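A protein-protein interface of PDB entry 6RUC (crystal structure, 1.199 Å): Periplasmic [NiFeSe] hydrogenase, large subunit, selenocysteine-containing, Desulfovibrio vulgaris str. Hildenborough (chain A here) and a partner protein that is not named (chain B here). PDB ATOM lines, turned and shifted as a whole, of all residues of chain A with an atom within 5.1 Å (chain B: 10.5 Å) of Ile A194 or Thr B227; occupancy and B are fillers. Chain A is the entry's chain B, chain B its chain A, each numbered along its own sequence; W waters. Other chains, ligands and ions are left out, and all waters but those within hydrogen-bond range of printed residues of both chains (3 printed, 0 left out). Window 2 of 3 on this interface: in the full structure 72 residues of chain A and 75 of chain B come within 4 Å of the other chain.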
ATOM      1  N   ASN A  98      31.852 -18.697 -13.077  1.00  0.00           N
ATOM      2  CA  ASN A  98      31.128 -18.031 -11.995  1.00  0.00           C
ATOM      3  C   ASN A  98      29.722 -18.588 -11.820  1.00  0.00           C
ATOM      4  O   ASN A  98      29.185 -18.551 -10.701  1.00  0.00           O
ATOM      5  CB  ASN A  98      31.082 -16.521 -12.221  1.00  0.00           C
ATOM      6  CG  ASN A  98      31.171 -15.738 -10.926  1.00  0.00           C
ATOM      7  OD1 ASN A  98      32.011 -16.021 -10.059  1.00  0.00           O
ATOM      8  ND2 ASN A  98      30.306 -14.741 -10.779  1.00  0.00           N
ATOM      9  N   ALA A 191      23.418 -19.966 -14.311  1.00  0.00           N
ATOM     10  CA  ALA A 191      22.583 -19.359 -13.286  1.00  0.00           C
ATOM     11  C   ALA A 191      22.107 -18.007 -13.806  1.00  0.00           C
ATOM     12  O   ALA A 191      22.856 -17.283 -14.473  1.00  0.00           O
ATOM     13  CB  ALA A 191      23.362 -19.210 -11.976  1.00  0.00           C
ATOM     14  N   THR A 192      20.858 -17.664 -13.491  1.00  0.00           N
ATOM     15  CA  THR A 192      20.184 -16.549 -14.150  1.00  0.00           C
ATOM     16  C   THR A 192      20.518 -15.184 -13.563  1.00  0.00           C
ATOM     17  O   THR A 192      20.144 -14.172 -14.171  1.00  0.00           O
ATOM     18  CB  THR A 192      18.666 -16.727 -14.067  1.00  0.00           C
ATOM     19  OG1 THR A 192      18.278 -16.785 -12.696  1.00  0.00           O
ATOM     20  CG2 THR A 192      18.197 -17.958 -14.790  1.00  0.00           C
ATOM     21  N   GLU A 193      21.173 -15.129 -12.403  1.00  0.00           N
ATOM     22  CA  GLU A 193      21.426 -13.869 -11.712  1.00  0.00           C
ATOM     23  C   GLU A 193      22.866 -13.822 -11.211  1.00  0.00           C
ATOM     24  O   GLU A 193      23.269 -14.627 -10.362  1.00  0.00           O
ATOM     25  CB  GLU A 193      20.433 -13.673 -10.556  1.00  0.00           C
ATOM     26  CG  GLU A 193      20.708 -12.398  -9.747  1.00  0.00           C
ATOM     27  CD  GLU A 193      19.735 -12.144  -8.629  1.00  0.00           C
ATOM     28  OE1 GLU A 193      18.705 -12.826  -8.545  1.00  0.00           O
ATOM     29  OE2 GLU A 193      20.003 -11.225  -7.827  1.00  0.00           O
ATOM     30  N   ILE A 194      23.623 -12.857 -11.722  1.00  0.00           N
ATOM     31  CA  ILE A 194      25.001 -12.623 -11.282  1.00  0.00           C
ATOM     32  C   ILE A 194      24.986 -12.182  -9.823  1.00  0.00           C
ATOM     33  O   ILE A 194      24.288 -11.210  -9.486  1.00  0.00           O
ATOM     34  CB  ILE A 194      25.630 -11.526 -12.155  1.00  0.00           C
ATOM     35  CG1 ILE A 194      25.819 -12.044 -13.583  1.00  0.00           C
ATOM     36  CG2 ILE A 194      26.931 -11.039 -11.565  1.00  0.00           C
ATOM     37  CD1 ILE A 194      26.151 -10.963 -14.594  1.00  0.00           C
ATOM     38  N   PRO A 195      25.760 -12.808  -8.932  1.00  0.00           N
ATOM     39  CA  PRO A 195      25.850 -12.304  -7.551  1.00  0.00           C
ATOM     40  C   PRO A 195      26.493 -10.924  -7.478  1.00  0.00           C
ATOM     41  O   PRO A 195      27.568 -10.690  -8.043  1.00  0.00           O
ATOM     42  CB  PRO A 195      26.718 -13.356  -6.846  1.00  0.00           C
ATOM     43  CG  PRO A 195      26.471 -14.611  -7.613  1.00  0.00           C
ATOM     44  CD  PRO A 195      26.399 -14.134  -9.059  1.00  0.00           C
ATOM     45  N   THR A 196      25.836 -10.014  -6.752  1.00  0.00           N
ATOM     46  CA  THR A 196      26.381  -8.689  -6.460  1.00  0.00           C
ATOM     47  C   THR A 196      27.096  -8.696  -5.105  1.00  0.00           C
ATOM     48  O   THR A 196      26.860  -9.565  -4.256  1.00  0.00           O
ATOM     49  CB  THR A 196      25.266  -7.644  -6.418  1.00  0.00           C
ATOM     50  OG1 THR A 196      24.396  -7.912  -5.308  1.00  0.00           O
ATOM     51  CG2 THR A 196      24.459  -7.632  -7.727  1.00  0.00           C
ATOM     52  N   ALA A 395      32.013 -11.298  -7.613  1.00  0.00           N
ATOM     53  CA  ALA A 395      30.866 -10.426  -7.803  1.00  0.00           C
ATOM     54  C   ALA A 395      30.923  -9.789  -9.185  1.00  0.00           C
ATOM     55  O   ALA A 395      31.985  -9.372  -9.650  1.00  0.00           O
ATOM     56  CB  ALA A 395      30.851  -9.328  -6.741  1.00  0.00           C
ATOM     57  N   GLY A 396      29.777  -9.745  -9.861  1.00  0.00           N
ATOM     58  CA  GLY A 396      29.665  -9.065 -11.133  1.00  0.00           C
ATOM     59  C   GLY A 396      30.016  -9.873 -12.363  1.00  0.00           C
ATOM     60  O   GLY A 396      29.730  -9.418 -13.475  1.00  0.00           O
ATOM     61  N   GLU A 397      30.609 -11.054 -12.214  1.00  0.00           N
ATOM     62  CA  GLU A 397      31.046 -11.838 -13.362  1.00  0.00           C
ATOM     63  C   GLU A 397      29.904 -12.712 -13.875  1.00  0.00           C
ATOM     64  O   GLU A 397      29.155 -13.316 -13.098  1.00  0.00           O
ATOM     65  CB  GLU A 397      32.264 -12.690 -13.004  1.00  0.00           C
ATOM     66  CG  GLU A 397      33.532 -11.888 -12.777  1.00  0.00           C
ATOM     67  CD  GLU A 397      33.988 -11.162 -14.022  1.00  0.00           C
ATOM     68  OE1 GLU A 397      34.100 -11.815 -15.076  1.00  0.00           O
ATOM     69  OE2 GLU A 397      34.213  -9.937 -13.953  1.00  0.00           O
ATOM     70  N   ASP A 398      29.765 -12.769 -15.197  1.00  0.00           N
ATOM     71  CA  ASP A 398      28.595 -13.407 -15.804  1.00  0.00           C
ATOM     72  C   ASP A 398      28.495 -14.886 -15.421  1.00  0.00           C
ATOM     73  O   ASP A 398      29.495 -15.597 -15.268  1.00  0.00           O
ATOM     74  CB  ASP A 398      28.607 -13.229 -17.333  1.00  0.00           C
ATOM     75  CG  ASP A 398      27.191 -13.275 -17.971  1.00  0.00           C
ATOM     76  OD1 ASP A 398      26.188 -13.681 -17.322  1.00  0.00           O
ATOM     77  OD2 ASP A 398      27.088 -12.890 -19.163  1.00  0.00           O
ATOM     78  N   THR A 399      27.258 -15.346 -15.268  1.00  0.00           N
ATOM     79  CA  THR A 399      26.951 -16.674 -14.771  1.00  0.00           C
ATOM     80  C   THR A 399      26.194 -17.550 -15.764  1.00  0.00           C
ATOM     81  O   THR A 399      25.885 -18.696 -15.424  1.00  0.00           O
ATOM     82  CB  THR A 399      26.111 -16.551 -13.494  1.00  0.00           C
ATOM     83  OG1 THR A 399      25.007 -15.673 -13.735  1.00  0.00           O
ATOM     84  CG2 THR A 399      26.954 -16.006 -12.345  1.00  0.00           C
ATOM     85  N   VAL A 400      25.861 -17.057 -16.964  1.00  0.00           N
ATOM     86  CA  VAL A 400      25.010 -17.811 -17.878  1.00  0.00           C
ATOM     87  C   VAL A 400      25.469 -17.615 -19.317  1.00  0.00           C
ATOM     88  O   VAL A 400      25.974 -16.550 -19.700  1.00  0.00           O
ATOM     89  CB  VAL A 400      23.500 -17.452 -17.700  1.00  0.00           C
ATOM     90  CG1 VAL A 400      23.083 -16.252 -18.588  1.00  0.00           C
ATOM     91  CG2 VAL A 400      22.620 -18.649 -17.965  1.00  0.00           C
ATOM     92  N   TYR B 213       9.584  -3.352 -14.342  1.00  0.00           N
ATOM     93  CA  TYR B 213      10.175  -3.285 -15.673  1.00  0.00           C
ATOM     94  C   TYR B 213       9.162  -2.913 -16.746  1.00  0.00           C
ATOM     95  O   TYR B 213       9.481  -2.991 -17.935  1.00  0.00           O
ATOM     96  CB  TYR B 213      10.905  -4.602 -15.999  1.00  0.00           C
ATOM     97  CG  TYR B 213      11.790  -5.012 -14.842  1.00  0.00           C
ATOM     98  CD1 TYR B 213      12.899  -4.257 -14.461  1.00  0.00           C
ATOM     99  CD2 TYR B 213      11.474  -6.123 -14.074  1.00  0.00           C
ATOM    100  CE1 TYR B 213      13.684  -4.632 -13.352  1.00  0.00           C
ATOM    101  CE2 TYR B 213      12.248  -6.497 -12.987  1.00  0.00           C
ATOM    102  CZ  TYR B 213      13.338  -5.748 -12.625  1.00  0.00           C
ATOM    103  OH  TYR B 213      14.083  -6.141 -11.525  1.00  0.00           O
ATOM    104  N   MET B 222      14.194  -5.231 -24.326  1.00  0.00           N
ATOM    105  CA  MET B 222      14.079  -6.609 -23.858  1.00  0.00           C
ATOM    106  C   MET B 222      15.455  -7.192 -23.592  1.00  0.00           C
ATOM    107  O   MET B 222      16.357  -7.084 -24.431  1.00  0.00           O
ATOM    108  CB  MET B 222      13.421  -7.490 -24.926  1.00  0.00           C
ATOM    109  CG  MET B 222      12.030  -7.075 -25.278  1.00  0.00           C
ATOM    110  SD  MET B 222      10.936  -7.334 -23.876  1.00  0.00           S
ATOM    111  CE  MET B 222       9.464  -6.526 -24.489  1.00  0.00           C
ATOM    112  N   SER B 223      15.600  -7.857 -22.455  1.00  0.00           N
ATOM    113  CA  SER B 223      16.834  -8.578 -22.186  1.00  0.00           C
ATOM    114  C   SER B 223      16.981  -9.782 -23.116  1.00  0.00           C
ATOM    115  O   SER B 223      16.020 -10.518 -23.372  1.00  0.00           O
ATOM    116  CB  SER B 223      16.846  -9.022 -20.727  1.00  0.00           C
ATOM    117  OG  SER B 223      16.958  -7.867 -19.905  1.00  0.00           O
ATOM    118  N   ALA B 224      18.200  -9.984 -23.623  1.00  0.00           N
ATOM    119  CA  ALA B 224      18.508 -11.145 -24.448  1.00  0.00           C
ATOM    120  C   ALA B 224      19.224 -12.255 -23.690  1.00  0.00           C
ATOM    121  O   ALA B 224      19.359 -13.362 -24.221  1.00  0.00           O
ATOM    122  CB  ALA B 224      19.367 -10.742 -25.643  1.00  0.00           C
ATOM    123  N   THR B 225      19.702 -11.980 -22.487  1.00  0.00           N
ATOM    124  CA  THR B 225      20.263 -12.986 -21.607  1.00  0.00           C
ATOM    125  C   THR B 225      19.654 -12.781 -20.232  1.00  0.00           C
ATOM    126  O   THR B 225      19.324 -11.653 -19.857  1.00  0.00           O
ATOM    127  CB  THR B 225      21.780 -12.895 -21.496  1.00  0.00           C
ATOM    128  OG1 THR B 225      22.217 -13.820 -20.487  1.00  0.00           O
ATOM    129  CG2 THR B 225      22.240 -11.486 -21.141  1.00  0.00           C
ATOM    130  N   PHE B 226      19.484 -13.883 -19.494  1.00  0.00           N
ATOM    131  CA  PHE B 226      18.852 -13.797 -18.184  1.00  0.00           C
ATOM    132  C   PHE B 226      19.585 -12.835 -17.266  1.00  0.00           C
ATOM    133  O   PHE B 226      18.958 -12.194 -16.418  1.00  0.00           O
ATOM    134  CB  PHE B 226      18.816 -15.166 -17.500  1.00  0.00           C
ATOM    135  CG  PHE B 226      17.898 -16.164 -18.152  1.00  0.00           C
ATOM    136  CD1 PHE B 226      16.520 -16.031 -18.035  1.00  0.00           C
ATOM    137  CD2 PHE B 226      18.407 -17.251 -18.833  1.00  0.00           C
ATOM    138  CE1 PHE B 226      15.669 -16.949 -18.639  1.00  0.00           C
ATOM    139  CE2 PHE B 226      17.564 -18.166 -19.431  1.00  0.00           C
ATOM    140  CZ  PHE B 226      16.197 -18.023 -19.330  1.00  0.00           C
ATOM    141  N   THR B 227      20.897 -12.715 -17.409  1.00  0.00           N
ATOM    142  CA  THR B 227      21.668 -11.941 -16.444  1.00  0.00           C
ATOM    143  C   THR B 227      21.625 -10.438 -16.707  1.00  0.00           C
ATOM    144  O   THR B 227      22.170  -9.676 -15.899  1.00  0.00           O
ATOM    145  CB  THR B 227      23.113 -12.453 -16.371  1.00  0.00           C
ATOM    146  OG1 THR B 227      23.679 -12.501 -17.686  1.00  0.00           O
ATOM    147  CG2 THR B 227      23.169 -13.837 -15.723  1.00  0.00           C
ATOM    148  N   ASP B 228      20.985  -9.998 -17.791  1.00  0.00           N
ATOM    149  CA  ASP B 228      20.745  -8.577 -18.059  1.00  0.00           C
ATOM    150  C   ASP B 228      19.509  -8.180 -17.274  1.00  0.00           C
ATOM    151  O   ASP B 228      18.383  -8.518 -17.651  1.00  0.00           O
ATOM    152  CB  ASP B 228      20.525  -8.341 -19.553  1.00  0.00           C
ATOM    153  CG  ASP B 228      20.122  -6.904 -19.888  1.00  0.00           C
ATOM    154  OD1 ASP B 228      19.893  -6.078 -18.972  1.00  0.00           O
ATOM    155  OD2 ASP B 228      20.053  -6.597 -21.101  1.00  0.00           O
ATOM    156  N   LYS B 229      19.709  -7.468 -16.174  1.00  0.00           N
ATOM    157  CA  LYS B 229      18.599  -7.105 -15.298  1.00  0.00           C
ATOM    158  C   LYS B 229      17.986  -5.745 -15.623  1.00  0.00           C
ATOM    159  O   LYS B 229      17.070  -5.303 -14.909  1.00  0.00           O
ATOM    160  CB  LYS B 229      19.038  -7.180 -13.826  1.00  0.00           C
ATOM    161  CG  LYS B 229      19.558  -8.560 -13.386  1.00  0.00           C
ATOM    162  CD  LYS B 229      18.638  -9.692 -13.842  1.00  0.00           C
ATOM    163  CE  LYS B 229      18.932 -11.002 -13.145  1.00  0.00           C
ATOM    164  NZ  LYS B 229      18.149 -12.099 -13.746  1.00  0.00           N
ATOM    165  N   VAL B 230      18.457  -5.086 -16.681  1.00  0.00           N
ATOM    166  CA  VAL B 230      17.907  -3.783 -17.052  1.00  0.00           C
ATOM    167  C   VAL B 230      16.629  -3.932 -17.876  1.00  0.00           C
ATOM    168  O   VAL B 230      15.654  -3.190 -17.677  1.00  0.00           O
ATOM    169  CB  VAL B 230      18.968  -2.947 -17.800  1.00  0.00           C
ATOM    170  CG1 VAL B 230      18.347  -1.666 -18.396  1.00  0.00           C
ATOM    171  CG2 VAL B 230      20.131  -2.599 -16.868  1.00  0.00           C
ATOM    172  N   GLY B 231      16.625  -4.840 -18.842  1.00  0.00           N
ATOM    173  CA  GLY B 231      15.507  -4.957 -19.754  1.00  0.00           C
ATOM    174  C   GLY B 231      14.337  -5.750 -19.190  1.00  0.00           C
ATOM    175  O   GLY B 231      14.429  -6.411 -18.155  1.00  0.00           O
ATOM    176  N   CYS B 232      13.221  -5.666 -19.909  1.00  0.00           N
ATOM    177  CA  CYS B 232      12.062  -6.500 -19.627  1.00  0.00           C
ATOM    178  C   CYS B 232      12.381  -7.954 -19.993  1.00  0.00           C
ATOM    179  O   CYS B 232      13.186  -8.234 -20.892  1.00  0.00           O
ATOM    180  CB  CYS B 232      10.868  -5.960 -20.421  1.00  0.00           C
ATOM    181  SG  CYS B 232       9.418  -7.051 -20.569  1.00  0.00           S
ATOM    182  N   ARG B 233      11.741  -8.880 -19.281  1.00  0.00           N
ATOM    183  CA  ARG B 233      11.955 -10.318 -19.402  1.00  0.00           C
ATOM    184  C   ARG B 233      10.970 -11.000 -20.360  1.00  0.00           C
ATOM    185  O   ARG B 233      10.981 -12.232 -20.463  1.00  0.00           O
ATOM    186  CB  ARG B 233      11.855 -10.960 -18.012  1.00  0.00           C
ATOM    187  CG  ARG B 233      13.028 -10.686 -17.064  1.00  0.00           C
ATOM    188  CD  ARG B 233      13.146  -9.241 -16.566  1.00  0.00           C
ATOM    189  NE  ARG B 233      13.895  -9.232 -15.314  1.00  0.00           N
ATOM    190  CZ  ARG B 233      14.673  -8.257 -14.857  1.00  0.00           C
ATOM    191  NH1 ARG B 233      14.846  -7.129 -15.539  1.00  0.00           N
ATOM    192  NH2 ARG B 233      15.303  -8.433 -13.701  1.00  0.00           N
ATOM    193  N   LEU B 236      12.366 -13.464 -22.900  1.00  0.00           N
ATOM    194  CA  LEU B 236      12.899 -14.622 -22.192  1.00  0.00           C
ATOM    195  C   LEU B 236      11.811 -15.555 -21.693  1.00  0.00           C
ATOM    196  O   LEU B 236      12.152 -16.590 -21.119  1.00  0.00           O
ATOM    197  CB  LEU B 236      13.780 -14.161 -21.019  1.00  0.00           C
ATOM    198  CG  LEU B 236      15.073 -13.436 -21.388  1.00  0.00           C
ATOM    199  CD1 LEU B 236      15.645 -12.702 -20.184  1.00  0.00           C
ATOM    200  CD2 LEU B 236      16.086 -14.421 -21.946  1.00  0.00           C
ATOM    201  N   VAL B 256      13.863 -11.351  -0.158  1.00  0.00           N
ATOM    202  CA  VAL B 256      15.211 -11.318  -0.727  1.00  0.00           C
ATOM    203  C   VAL B 256      15.241 -11.377  -2.253  1.00  0.00           C
ATOM    204  O   VAL B 256      16.279 -11.063  -2.850  1.00  0.00           O
ATOM    205  CB  VAL B 256      16.128 -12.412  -0.139  1.00  0.00           C
ATOM    206  CG1 VAL B 256      16.229 -12.294   1.379  1.00  0.00           C
ATOM    207  CG2 VAL B 256      15.696 -13.835  -0.553  1.00  0.00           C
ATOM    208  N   ASN B 257      14.157 -11.787  -2.899  1.00  0.00           N
ATOM    209  CA  ASN B 257      14.146 -11.920  -4.351  1.00  0.00           C
ATOM    210  C   ASN B 257      12.711 -12.186  -4.791  1.00  0.00           C
ATOM    211  O   ASN B 257      11.814 -12.373  -3.964  1.00  0.00           O
ATOM    212  CB  ASN B 257      15.069 -13.067  -4.792  1.00  0.00           C
ATOM    213  CG  ASN B 257      15.748 -12.800  -6.140  1.00  0.00           C
ATOM    214  OD1 ASN B 257      15.236 -12.070  -6.984  1.00  0.00           O
ATOM    215  ND2 ASN B 257      16.915 -13.391  -6.331  1.00  0.00           N
ATOM    216  N   CYS B 259      10.603 -13.925  -8.690  1.00  0.00           N
ATOM    217  CA  CYS B 259      10.885 -14.656  -9.921  1.00  0.00           C
ATOM    218  C   CYS B 259      11.255 -13.732 -11.063  1.00  0.00           C
ATOM    219  O   CYS B 259      12.157 -14.047 -11.851  1.00  0.00           O
ATOM    220  CB  CYS B 259       9.680 -15.485 -10.317  1.00  0.00           C
ATOM    221  SG  CYS B 259       9.114 -16.566  -8.977  1.00  0.00           S
ATOM    222  N   VAL B 260      10.580 -12.582 -11.182  1.00  0.00           N
ATOM    223  CA  VAL B 260      10.850 -11.681 -12.304  1.00  0.00           C
ATOM    224  C   VAL B 260      12.222 -11.037 -12.167  1.00  0.00           C
ATOM    225  O   VAL B 260      12.939 -10.869 -13.156  1.00  0.00           O
ATOM    226  CB  VAL B 260       9.721 -10.644 -12.445  1.00  0.00           C
ATOM    227  CG1 VAL B 260      10.065  -9.588 -13.503  1.00  0.00           C
ATOM    228  CG2 VAL B 260       8.427 -11.329 -12.815  1.00  0.00           C
ATOM    229  N   GLN B 261      12.607 -10.625 -10.952  1.00  0.00           N
ATOM    230  CA  GLN B 261      13.946 -10.067 -10.792  1.00  0.00           C
ATOM    231  C   GLN B 261      15.005 -11.097 -11.160  1.00  0.00           C
ATOM    232  O   GLN B 261      15.987 -10.777 -11.842  1.00  0.00           O
ATOM    233  CB  GLN B 261      14.155  -9.586  -9.352  1.00  0.00           C
ATOM    234  CG  GLN B 261      15.348  -8.638  -9.148  1.00  0.00           C
ATOM    235  CD  GLN B 261      16.724  -9.269  -9.286  1.00  0.00           C
ATOM    236  OE1 GLN B 261      17.627  -8.694  -9.919  1.00  0.00           O
ATOM    237  NE2 GLN B 261      16.913 -10.419  -8.667  1.00  0.00           N
ATOM    238  N   ASN B 262      14.813 -12.342 -10.719  1.00  0.00           N
ATOM    239  CA  ASN B 262      15.828 -13.382 -10.789  1.00  0.00           C
ATOM    240  C   ASN B 262      15.891 -14.028 -12.164  1.00  0.00           C
ATOM    241  O   ASN B 262      16.977 -14.398 -12.622  1.00  0.00           O
ATOM    242  CB  ASN B 262      15.510 -14.437  -9.720  1.00  0.00           C
ATOM    243  CG  ASN B 262      16.424 -15.648  -9.766  1.00  0.00           C
ATOM    244  OD1 ASN B 262      15.987 -16.744 -10.087  1.00  0.00           O
ATOM    245  ND2 ASN B 262      17.703 -15.456  -9.424  1.00  0.00           N
ATOM    246  N   ALA B 263      14.738 -14.213 -12.806  1.00  0.00           N
ATOM    247  CA  ALA B 263      14.623 -14.982 -14.044  1.00  0.00           C
ATOM    248  C   ALA B 263      13.359 -14.521 -14.765  1.00  0.00           C
ATOM    249  O   ALA B 263      13.337 -13.405 -15.294  1.00  0.00           O
ATOM    250  CB  ALA B 263      14.628 -16.486 -13.754  1.00  0.00           C
ATOM    251  N   VAL B 264      12.291 -15.338 -14.760  1.00  0.00           N
ATOM    252  CA  VAL B 264      11.008 -14.992 -15.366  1.00  0.00           C
ATOM    253  C   VAL B 264       9.895 -15.485 -14.450  1.00  0.00           C
ATOM    254  O   VAL B 264      10.087 -16.412 -13.665  1.00  0.00           O
ATOM    255  CB  VAL B 264      10.814 -15.628 -16.768  1.00  0.00           C
ATOM    256  CG1 VAL B 264      11.907 -15.181 -17.730  1.00  0.00           C
ATOM    257  CG2 VAL B 264      10.763 -17.161 -16.687  1.00  0.00           C
HETATM  258  O   HOH W   1      20.353  -8.829  -9.376  1.00  0.00           O
HETATM  259  O   HOH W   2      24.989 -14.050 -20.646  1.00  0.00           O
HETATM  260  O   HOH W   3      22.379 -10.771 -13.300  1.00  0.00           O
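The side-chain carboxylate of Asp A398 is in hydrogen-bond range of the side-chain hydroxyl of Thr B227 (2.8 Å).
The side-chain amino group (NZ) of Lys B229 sits at hydrogen-bond distance from the backbone carbonyl oxygen (O) of Thr A192, 2.9 Å away.
The side-chain carboxylate of Glu A193 sits at hydrogen-bond distance from the side-chain amide nitrogen of Asn B257 (2.9 Å).
The side-chain amide nitrogen of Gln B261 is in hydrogen-bond range of the side-chain carboxylate of Glu A193 (3.0 Å).
The side-chain hydroxyl of Thr A192 lies within hydrogen-bond range of the backbone carbonyl oxygen of Asn B262, at 2.7 Å.
The side-chain amide nitrogen of Asn B262 is in hydrogen-bond range of the side-chain carboxylate of Glu A193, 2.9 Å away.
The backbone carbonyl oxygen (O) of Phe B226 lies close to the backbone carbonyl oxygen (O) of Thr A192, 3.2 Å away.
The side-chain hydroxyl (OG1) of Thr B227 sits at hydrogen-bond distance from the side-chain hydroxyl (OG1) of Thr B225, 3.4 Å away.
The side-chain amino group (NZ) of Lys B229 is in hydrogen-bond range of the backbone carbonyl oxygen (O) of Phe B226 (2.8 Å).
O of Lys B229 is in hydrogen-bond range of NH1 of Arg B233 (2.9 Å).
The side-chain amino group (NZ) of Lys B229 is in hydrogen-bond range of the backbone carbonyl oxygen (O) of Asn B262, 2.8 Å away.
The side-chain amide oxygen (OD1) of Asn B257 is in hydrogen-bond range of the side-chain amide nitrogen (NE2) of Gln B261, 2.9 Å away.
N of Val A400 lies within hydrogen-bond range of OD1 of Asp A398 (3.4 Å).
Among the printed residues, pairs that only touch across the chains: Val A400 with Thr B225 (3.2 Å), Thr A399 with Thr B227 (3.3 Å), Thr A192 with Thr B227 (3.4 Å), Ala A191 with Thr B227 (3.7 Å), Val A400 with Thr B227 (3.7 Å), Thr A192 with Ala B263 (3.8 Å) and Ile A194 with Thr B227 (3.8 Å).
Of the printed residues of chain B, Glu A193 touches Asn B257, Gln B261 and Asn B262.
No residue of chain B comes within 4 Å of Thr A196.
Printed residues of chain B within 4 Å of Asp A398: Thr B227.
Thr A399 touches just one residue of chain B: Thr B227.
Printed residues of chain A within 4 Å of Thr B227: Ala A191 (3.7 Å), Thr A192 (3.4 Å), Ile A194 (3.8 Å), Asp A398 (2.8 Å), Thr A399 (3.3 Å) and Val A400 (3.7 Å).
Of the printed residues of chain A, Lys B229 touches Thr A192 (2.9 Å).
Leu B236 touches none of the printed residues of chain A.
Printed residues of chain A within 4 Å of Asn B257: Glu A193.
Printed residues of chain A within 4 Å of Gln B261: Glu A193.
Of the printed residues of chain A, Ala B263 touches Thr A192 (3.8 Å).
The nearest residue of chain B that does not touch Ile A194 is Lys B229 (5.2 Å).
The nearest residue of chain A that does not touch Thr B227 is Glu A193 (4.1 Å).
The nearest printed residue of chain A that does not touch Phe B226 is Val A400 (4.4 Å).
Hydrophobic or aromatic side chains of chain A within 4 Å of the printed part of chain B: Ile A194 and Val A400.
Water W1 lies within hydrogen-bond range of OE1 of Gln B261 (2.8 Å) and OE2 of Glu A193 (2.9 Å).
Water W2 lies within hydrogen-bond range of OG1 of Thr B225 (2.8 Å), OD2 of Asp A398 (2.8 Å) and O of Val A400 (2.8 Å).
Water W3 bridges the backbone carbonyl oxygen (O) of Thr B227 (2.8 Å) and the backbone NH (N) of Ile A194 (2.9 Å).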
